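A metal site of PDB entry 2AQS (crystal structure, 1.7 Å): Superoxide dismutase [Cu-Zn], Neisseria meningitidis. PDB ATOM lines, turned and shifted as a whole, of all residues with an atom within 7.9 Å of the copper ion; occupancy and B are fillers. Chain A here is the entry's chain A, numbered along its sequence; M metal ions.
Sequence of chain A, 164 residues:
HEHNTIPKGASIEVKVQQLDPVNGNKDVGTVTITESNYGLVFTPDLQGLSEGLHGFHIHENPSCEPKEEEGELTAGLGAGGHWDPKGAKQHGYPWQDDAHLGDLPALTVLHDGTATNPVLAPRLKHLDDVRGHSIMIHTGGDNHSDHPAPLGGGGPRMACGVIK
ND1 of His 138 is in hydrogen-bond range of O of Pro 156 (3.2 Å). ND1 of His 59 lies close to O of Gly 81, at 3.3 Å. The side-chain carboxylate (OD2) of Asp 142 sits at hydrogen-bond distance from a ring nitrogen (NE2) of His 57 (2.9 Å). The backbone NH (N) of His 59 lies within hydrogen-bond range of the backbone carbonyl oxygen (O) of Ser 134, at 2.8 Å. The backbone NH (N) of His 138 sits at hydrogen-bond distance from the backbone carbonyl oxygen (O) of Gly 55 (2.9 Å). O of His 57 sits at hydrogen-bond distance from N of Met 136 (2.7 Å). A ring nitrogen (ND1) of His 138 lies within hydrogen-bond range of the backbone carbonyl oxygen (O) of Gly 155. NE2 of His 82 lies close to ND1 of His 57 (3.3 Å).
NE2 of His 82 touches the copper ion, 3.2 Å away. Met 136 touches the copper ion. Of the 25 residues printed, 5 come within 4 Å of the copper ion. The nearest printed residue that does not touch the copper ion is Phe 56 (5.2 Å).
The copper ion is bound by a ring nitrogen (NE2) of His 59 (2.0 Å), a ring nitrogen (NE2) of His 138 (2.0 Å) and a ring nitrogen (ND1) of His 57 (2.1 Å).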
ATOM      1  N   GLY A  55     -24.439  -2.904 -23.800  1.00  0.00           N
ATOM      2  CA  GLY A  55     -24.189  -2.538 -25.182  1.00  0.00           C
ATOM      3  C   GLY A  55     -22.790  -3.005 -25.542  1.00  0.00           C
ATOM      4  O   GLY A  55     -21.862  -2.851 -24.748  1.00  0.00           O
ATOM      5  N   PHE A  56     -22.641  -3.546 -26.740  1.00  0.00           N
ATOM      6  CA  PHE A  56     -21.371  -4.093 -27.180  1.00  0.00           C
ATOM      7  C   PHE A  56     -21.164  -3.661 -28.631  1.00  0.00           C
ATOM      8  O   PHE A  56     -21.908  -4.067 -29.505  1.00  0.00           O
ATOM      9  CB  PHE A  56     -21.489  -5.620 -27.036  1.00  0.00           C
ATOM     10  CG  PHE A  56     -20.222  -6.378 -27.290  1.00  0.00           C
ATOM     11  CD1 PHE A  56     -19.024  -5.970 -26.720  1.00  0.00           C
ATOM     12  CD2 PHE A  56     -20.258  -7.563 -28.019  1.00  0.00           C
ATOM     13  CE1 PHE A  56     -17.879  -6.732 -26.877  1.00  0.00           C
ATOM     14  CE2 PHE A  56     -19.125  -8.338 -28.178  1.00  0.00           C
ATOM     15  CZ  PHE A  56     -17.936  -7.929 -27.608  1.00  0.00           C
ATOM     16  N   HIS A  57     -20.172  -2.798 -28.872  1.00  0.00           N
ATOM     17  CA  HIS A  57     -19.910  -2.315 -30.226  1.00  0.00           C
ATOM     18  C   HIS A  57     -18.445  -2.093 -30.563  1.00  0.00           C
ATOM     19  O   HIS A  57     -17.596  -1.916 -29.681  1.00  0.00           O
ATOM     20  CB  HIS A  57     -20.607  -0.974 -30.500  1.00  0.00           C
ATOM     21  CG  HIS A  57     -21.811  -0.715 -29.639  1.00  0.00           C
ATOM     22  ND1 HIS A  57     -21.790   0.172 -28.587  1.00  0.00           N
ATOM     23  CD2 HIS A  57     -23.080  -1.192 -29.714  1.00  0.00           C
ATOM     24  CE1 HIS A  57     -22.984   0.223 -28.034  1.00  0.00           C
ATOM     25  NE2 HIS A  57     -23.795  -0.593 -28.699  1.00  0.00           N
ATOM     26  N   ILE A  58     -18.147  -2.101 -31.855  1.00  0.00           N
ATOM     27  CA  ILE A  58     -16.807  -1.828 -32.329  1.00  0.00           C
ATOM     28  C   ILE A  58     -16.789  -0.306 -32.512  1.00  0.00           C
ATOM     29  O   ILE A  58     -17.699   0.264 -33.120  1.00  0.00           O
ATOM     30  CB  ILE A  58     -16.530  -2.498 -33.703  1.00  0.00           C
ATOM     31  CG1 ILE A  58     -16.688  -4.018 -33.573  1.00  0.00           C
ATOM     32  CG2 ILE A  58     -15.156  -2.101 -34.206  1.00  0.00           C
ATOM     33  CD1 ILE A  58     -15.701  -4.696 -32.673  1.00  0.00           C
ATOM     34  N   HIS A  59     -15.775   0.350 -31.970  1.00  0.00           N
ATOM     35  CA  HIS A  59     -15.657   1.788 -32.100  1.00  0.00           C
ATOM     36  C   HIS A  59     -14.539   2.106 -33.081  1.00  0.00           C
ATOM     37  O   HIS A  59     -13.630   1.305 -33.279  1.00  0.00           O
ATOM     38  CB  HIS A  59     -15.441   2.448 -30.730  1.00  0.00           C
ATOM     39  CG  HIS A  59     -16.701   2.564 -29.923  1.00  0.00           C
ATOM     40  ND1 HIS A  59     -17.204   3.772 -29.490  1.00  0.00           N
ATOM     41  CD2 HIS A  59     -17.591   1.625 -29.513  1.00  0.00           C
ATOM     42  CE1 HIS A  59     -18.347   3.571 -28.849  1.00  0.00           C
ATOM     43  NE2 HIS A  59     -18.600   2.273 -28.856  1.00  0.00           N
ATOM     44  N   ALA A  79     -11.765   6.208 -27.949  1.00  0.00           N
ATOM     45  CA  ALA A  79     -12.169   5.220 -28.927  1.00  0.00           C
ATOM     46  C   ALA A  79     -13.001   5.833 -30.049  1.00  0.00           C
ATOM     47  O   ALA A  79     -13.183   5.223 -31.102  1.00  0.00           O
ATOM     48  CB  ALA A  79     -12.958   4.116 -28.248  1.00  0.00           C
ATOM     49  N   GLY A  80     -13.514   7.035 -29.833  1.00  0.00           N
ATOM     50  CA  GLY A  80     -14.334   7.666 -30.859  1.00  0.00           C
ATOM     51  C   GLY A  80     -15.745   7.099 -30.822  1.00  0.00           C
ATOM     52  O   GLY A  80     -16.140   6.483 -29.830  1.00  0.00           O
ATOM     53  N   GLY A  81     -16.491   7.298 -31.904  1.00  0.00           N
ATOM     54  CA  GLY A  81     -17.863   6.806 -31.947  1.00  0.00           C
ATOM     55  C   GLY A  81     -17.986   5.379 -32.475  1.00  0.00           C
ATOM     56  O   GLY A  81     -16.985   4.683 -32.667  1.00  0.00           O
ATOM     57  N   HIS A  82     -19.222   4.928 -32.680  1.00  0.00           N
ATOM     58  CA  HIS A  82     -19.436   3.590 -33.203  1.00  0.00           C
ATOM     59  C   HIS A  82     -18.805   3.495 -34.580  1.00  0.00           C
ATOM     60  O   HIS A  82     -18.941   4.412 -35.391  1.00  0.00           O
ATOM     61  CB  HIS A  82     -20.938   3.283 -33.319  1.00  0.00           C
ATOM     62  CG  HIS A  82     -21.635   3.143 -32.004  1.00  0.00           C
ATOM     63  ND1 HIS A  82     -22.868   2.551 -31.888  1.00  0.00           N
ATOM     64  CD2 HIS A  82     -21.278   3.527 -30.755  1.00  0.00           C
ATOM     65  CE1 HIS A  82     -23.255   2.574 -30.624  1.00  0.00           C
ATOM     66  NE2 HIS A  82     -22.309   3.164 -29.908  1.00  0.00           N
ATOM     67  N   TRP A  83     -18.109   2.395 -34.833  1.00  0.00           N
ATOM     68  CA  TRP A  83     -17.471   2.184 -36.129  1.00  0.00           C
ATOM     69  C   TRP A  83     -18.578   2.125 -37.198  1.00  0.00           C
ATOM     70  O   TRP A  83     -19.438   1.255 -37.170  1.00  0.00           O
ATOM     71  CB  TRP A  83     -16.689   0.876 -36.106  1.00  0.00           C
ATOM     72  CG  TRP A  83     -15.872   0.648 -37.329  1.00  0.00           C
ATOM     73  CD1 TRP A  83     -15.085   1.552 -37.977  1.00  0.00           C
ATOM     74  CD2 TRP A  83     -15.722  -0.590 -38.034  1.00  0.00           C
ATOM     75  NE1 TRP A  83     -14.450   0.956 -39.036  1.00  0.00           N
ATOM     76  CE2 TRP A  83     -14.825  -0.356 -39.099  1.00  0.00           C
ATOM     77  CE3 TRP A  83     -16.257  -1.874 -37.859  1.00  0.00           C
ATOM     78  CZ2 TRP A  83     -14.448  -1.363 -39.997  1.00  0.00           C
ATOM     79  CZ3 TRP A  83     -15.879  -2.881 -38.757  1.00  0.00           C
ATOM     80  CH2 TRP A  83     -14.989  -2.613 -39.809  1.00  0.00           C
ATOM     81  N   HIS A  91     -27.715   4.037 -35.378  1.00  0.00           N
ATOM     82  CA  HIS A  91     -27.498   2.840 -34.583  1.00  0.00           C
ATOM     83  C   HIS A  91     -28.632   1.847 -34.805  1.00  0.00           C
ATOM     84  O   HIS A  91     -29.806   2.239 -34.875  1.00  0.00           O
ATOM     85  CB  HIS A  91     -27.397   3.198 -33.101  1.00  0.00           C
ATOM     86  CG  HIS A  91     -27.108   2.030 -32.221  1.00  0.00           C
ATOM     87  ND1 HIS A  91     -25.880   1.398 -32.217  1.00  0.00           N
ATOM     88  CD2 HIS A  91     -27.881   1.360 -31.347  1.00  0.00           C
ATOM     89  CE1 HIS A  91     -25.916   0.378 -31.370  1.00  0.00           C
ATOM     90  NE2 HIS A  91     -27.121   0.338 -30.825  1.00  0.00           N
ATOM     91  N   GLY A 102     -20.368  -1.509 -36.779  1.00  0.00           N
ATOM     92  CA  GLY A 102     -19.825  -1.909 -35.491  1.00  0.00           C
ATOM     93  C   GLY A 102     -20.853  -2.325 -34.460  1.00  0.00           C
ATOM     94  O   GLY A 102     -20.482  -2.644 -33.328  1.00  0.00           O
ATOM     95  N   ASP A 103     -22.132  -2.361 -34.834  1.00  0.00           N
ATOM     96  CA  ASP A 103     -23.184  -2.730 -33.895  1.00  0.00           C
ATOM     97  C   ASP A 103     -23.269  -4.227 -33.688  1.00  0.00           C
ATOM     98  O   ASP A 103     -23.748  -4.966 -34.554  1.00  0.00           O
ATOM     99  CB  ASP A 103     -24.529  -2.172 -34.365  1.00  0.00           C
ATOM    100  CG  ASP A 103     -24.553  -0.653 -34.334  1.00  0.00           C
ATOM    101  OD1 ASP A 103     -23.668  -0.066 -33.685  1.00  0.00           O
ATOM    102  OD2 ASP A 103     -25.459  -0.045 -34.958  1.00  0.00           O
ATOM    103  N   SER A 134     -11.502  -0.582 -31.850  1.00  0.00           N
ATOM    104  CA  SER A 134     -11.673  -0.972 -30.457  1.00  0.00           C
ATOM    105  C   SER A 134     -13.024  -1.627 -30.240  1.00  0.00           C
ATOM    106  O   SER A 134     -13.929  -1.485 -31.048  1.00  0.00           O
ATOM    107  CB  SER A 134     -11.544   0.250 -29.540  1.00  0.00           C
ATOM    108  OG  SER A 134     -12.403   1.298 -29.938  1.00  0.00           O
ATOM    109  N   ILE A 135     -13.123  -2.378 -29.148  1.00  0.00           N
ATOM    110  CA  ILE A 135     -14.374  -3.034 -28.815  1.00  0.00           C
ATOM    111  C   ILE A 135     -14.808  -2.426 -27.483  1.00  0.00           C
ATOM    112  O   ILE A 135     -14.017  -2.325 -26.544  1.00  0.00           O
ATOM    113  CB  ILE A 135     -14.192  -4.579 -28.752  1.00  0.00           C
ATOM    114  CG1 ILE A 135     -15.545  -5.267 -28.634  1.00  0.00           C
ATOM    115  CG2 ILE A 135     -13.256  -4.974 -27.620  1.00  0.00           C
ATOM    116  CD1 ILE A 135     -15.499  -6.704 -29.081  1.00  0.00           C
ATOM    117  N   MET A 136     -16.069  -2.004 -27.422  1.00  0.00           N
ATOM    118  CA  MET A 136     -16.585  -1.325 -26.245  1.00  0.00           C
ATOM    119  C   MET A 136     -17.733  -2.035 -25.574  1.00  0.00           C
ATOM    120  O   MET A 136     -18.614  -2.575 -26.244  1.00  0.00           O
ATOM    121  CB  MET A 136     -17.032   0.085 -26.659  1.00  0.00           C
ATOM    122  CG  MET A 136     -17.210   1.086 -25.514  1.00  0.00           C
ATOM    123  SD  MET A 136     -15.627   1.614 -24.836  1.00  0.00           S
ATOM    124  CE  MET A 136     -14.996   2.616 -26.217  1.00  0.00           C
ATOM    125  N   ILE A 137     -17.731  -2.036 -24.247  1.00  0.00           N
ATOM    126  CA  ILE A 137     -18.806  -2.622 -23.460  1.00  0.00           C
ATOM    127  C   ILE A 137     -19.337  -1.458 -22.626  1.00  0.00           C
ATOM    128  O   ILE A 137     -18.597  -0.821 -21.878  1.00  0.00           O
ATOM    129  CB  ILE A 137     -18.301  -3.746 -22.517  1.00  0.00           C
ATOM    130  CG1 ILE A 137     -17.623  -4.850 -23.330  1.00  0.00           C
ATOM    131  CG2 ILE A 137     -19.495  -4.322 -21.752  1.00  0.00           C
ATOM    132  CD1 ILE A 137     -16.972  -5.931 -22.476  1.00  0.00           C
ATOM    133  N   HIS A 138     -20.622  -1.168 -22.788  1.00  0.00           N
ATOM    134  CA  HIS A 138     -21.257  -0.047 -22.100  1.00  0.00           C
ATOM    135  C   HIS A 138     -21.924  -0.371 -20.779  1.00  0.00           C
ATOM    136  O   HIS A 138     -22.234  -1.522 -20.469  1.00  0.00           O
ATOM    137  CB  HIS A 138     -22.278   0.598 -23.035  1.00  0.00           C
ATOM    138  CG  HIS A 138     -21.667   1.241 -24.247  1.00  0.00           C
ATOM    139  ND1 HIS A 138     -21.407   2.595 -24.316  1.00  0.00           N
ATOM    140  CD2 HIS A 138     -21.216   0.710 -25.401  1.00  0.00           C
ATOM    141  CE1 HIS A 138     -20.828   2.867 -25.483  1.00  0.00           C
ATOM    142  NE2 HIS A 138     -20.696   1.740 -26.156  1.00  0.00           N
ATOM    143  N   ASP A 142     -28.642  -2.209 -24.861  1.00  0.00           N
ATOM    144  CA  ASP A 142     -28.703  -1.835 -26.263  1.00  0.00           C
ATOM    145  C   ASP A 142     -30.027  -2.289 -26.866  1.00  0.00           C
ATOM    146  O   ASP A 142     -30.259  -3.491 -27.029  1.00  0.00           O
ATOM    147  CB  ASP A 142     -27.535  -2.506 -27.014  1.00  0.00           C
ATOM    148  CG  ASP A 142     -27.323  -1.925 -28.411  1.00  0.00           C
ATOM    149  OD1 ASP A 142     -28.244  -1.273 -28.941  1.00  0.00           O
ATOM    150  OD2 ASP A 142     -26.227  -2.143 -28.973  1.00  0.00           O
ATOM    151  N   LEU A 151     -27.794   5.812 -29.584  1.00  0.00           N
ATOM    152  CA  LEU A 151     -26.915   4.662 -29.532  1.00  0.00           C
ATOM    153  C   LEU A 151     -27.391   3.485 -28.665  1.00  0.00           C
ATOM    154  O   LEU A 151     -26.597   2.873 -27.944  1.00  0.00           O
ATOM    155  CB  LEU A 151     -25.519   5.126 -29.077  1.00  0.00           C
ATOM    156  CG  LEU A 151     -24.992   6.301 -29.923  1.00  0.00           C
ATOM    157  CD1 LEU A 151     -23.760   6.928 -29.265  1.00  0.00           C
ATOM    158  CD2 LEU A 151     -24.667   5.803 -31.325  1.00  0.00           C
ATOM    159  N   GLY A 154     -26.813   2.736 -24.530  1.00  0.00           N
ATOM    160  CA  GLY A 154     -25.606   2.220 -23.921  1.00  0.00           C
ATOM    161  C   GLY A 154     -24.984   3.171 -22.908  1.00  0.00           C
ATOM    162  O   GLY A 154     -24.434   2.737 -21.892  1.00  0.00           O
ATOM    163  N   GLY A 155     -25.072   4.462 -23.190  1.00  0.00           N
ATOM    164  CA  GLY A 155     -24.517   5.443 -22.267  1.00  0.00           C
ATOM    165  C   GLY A 155     -23.019   5.356 -22.080  1.00  0.00           C
ATOM    166  O   GLY A 155     -22.279   5.167 -23.055  1.00  0.00           O
ATOM    167  N   PRO A 156     -22.530   5.475 -20.837  1.00  0.00           N
ATOM    168  CA  PRO A 156     -21.100   5.414 -20.504  1.00  0.00           C
ATOM    169  C   PRO A 156     -20.370   4.156 -20.955  1.00  0.00           C
ATOM    170  O   PRO A 156     -20.959   3.090 -21.140  1.00  0.00           O
ATOM    171  CB  PRO A 156     -21.093   5.553 -18.983  1.00  0.00           C
ATOM    172  CG  PRO A 156     -22.311   6.392 -18.728  1.00  0.00           C
ATOM    173  CD  PRO A 156     -23.323   5.739 -19.629  1.00  0.00           C
ATOM    174  N   ARG A 157     -19.056   4.295 -21.086  1.00  0.00           N
ATOM    175  CA  ARG A 157     -18.209   3.193 -21.508  1.00  0.00           C
ATOM    176  C   ARG A 157     -17.678   2.511 -20.254  1.00  0.00           C
ATOM    177  O   ARG A 157     -16.924   3.097 -19.471  1.00  0.00           O
ATOM    178  CB  ARG A 157     -17.118   3.740 -22.416  1.00  0.00           C
ATOM    179  CG  ARG A 157     -17.779   4.432 -23.607  1.00  0.00           C
ATOM    180  CD  ARG A 157     -16.864   5.204 -24.539  1.00  0.00           C
ATOM    181  NE  ARG A 157     -17.669   5.881 -25.550  1.00  0.00           N
ATOM    182  CZ  ARG A 157     -17.216   6.380 -26.696  1.00  0.00           C
ATOM    183  NH1 ARG A 157     -15.927   6.279 -27.012  1.00  0.00           N
ATOM    184  NH2 ARG A 157     -18.065   6.935 -27.556  1.00  0.00           N
ATOM    185  N   ALA A 159     -16.209  -0.967 -20.167  1.00  0.00           N
ATOM    186  CA  ALA A 159     -14.983  -1.731 -20.401  1.00  0.00           C
ATOM    187  C   ALA A 159     -14.604  -1.561 -21.863  1.00  0.00           C
ATOM    188  O   ALA A 159     -15.456  -1.303 -22.708  1.00  0.00           O
ATOM    189  CB  ALA A 159     -15.207  -3.204 -20.079  1.00  0.00           C
HETATM  190 CU    CU M   1     -20.245   1.441 -28.088  1.00  0.00          CU
HETATM  191 ZN    ZN M   2     -24.109   1.797 -33.327  1.00  0.00          ZN
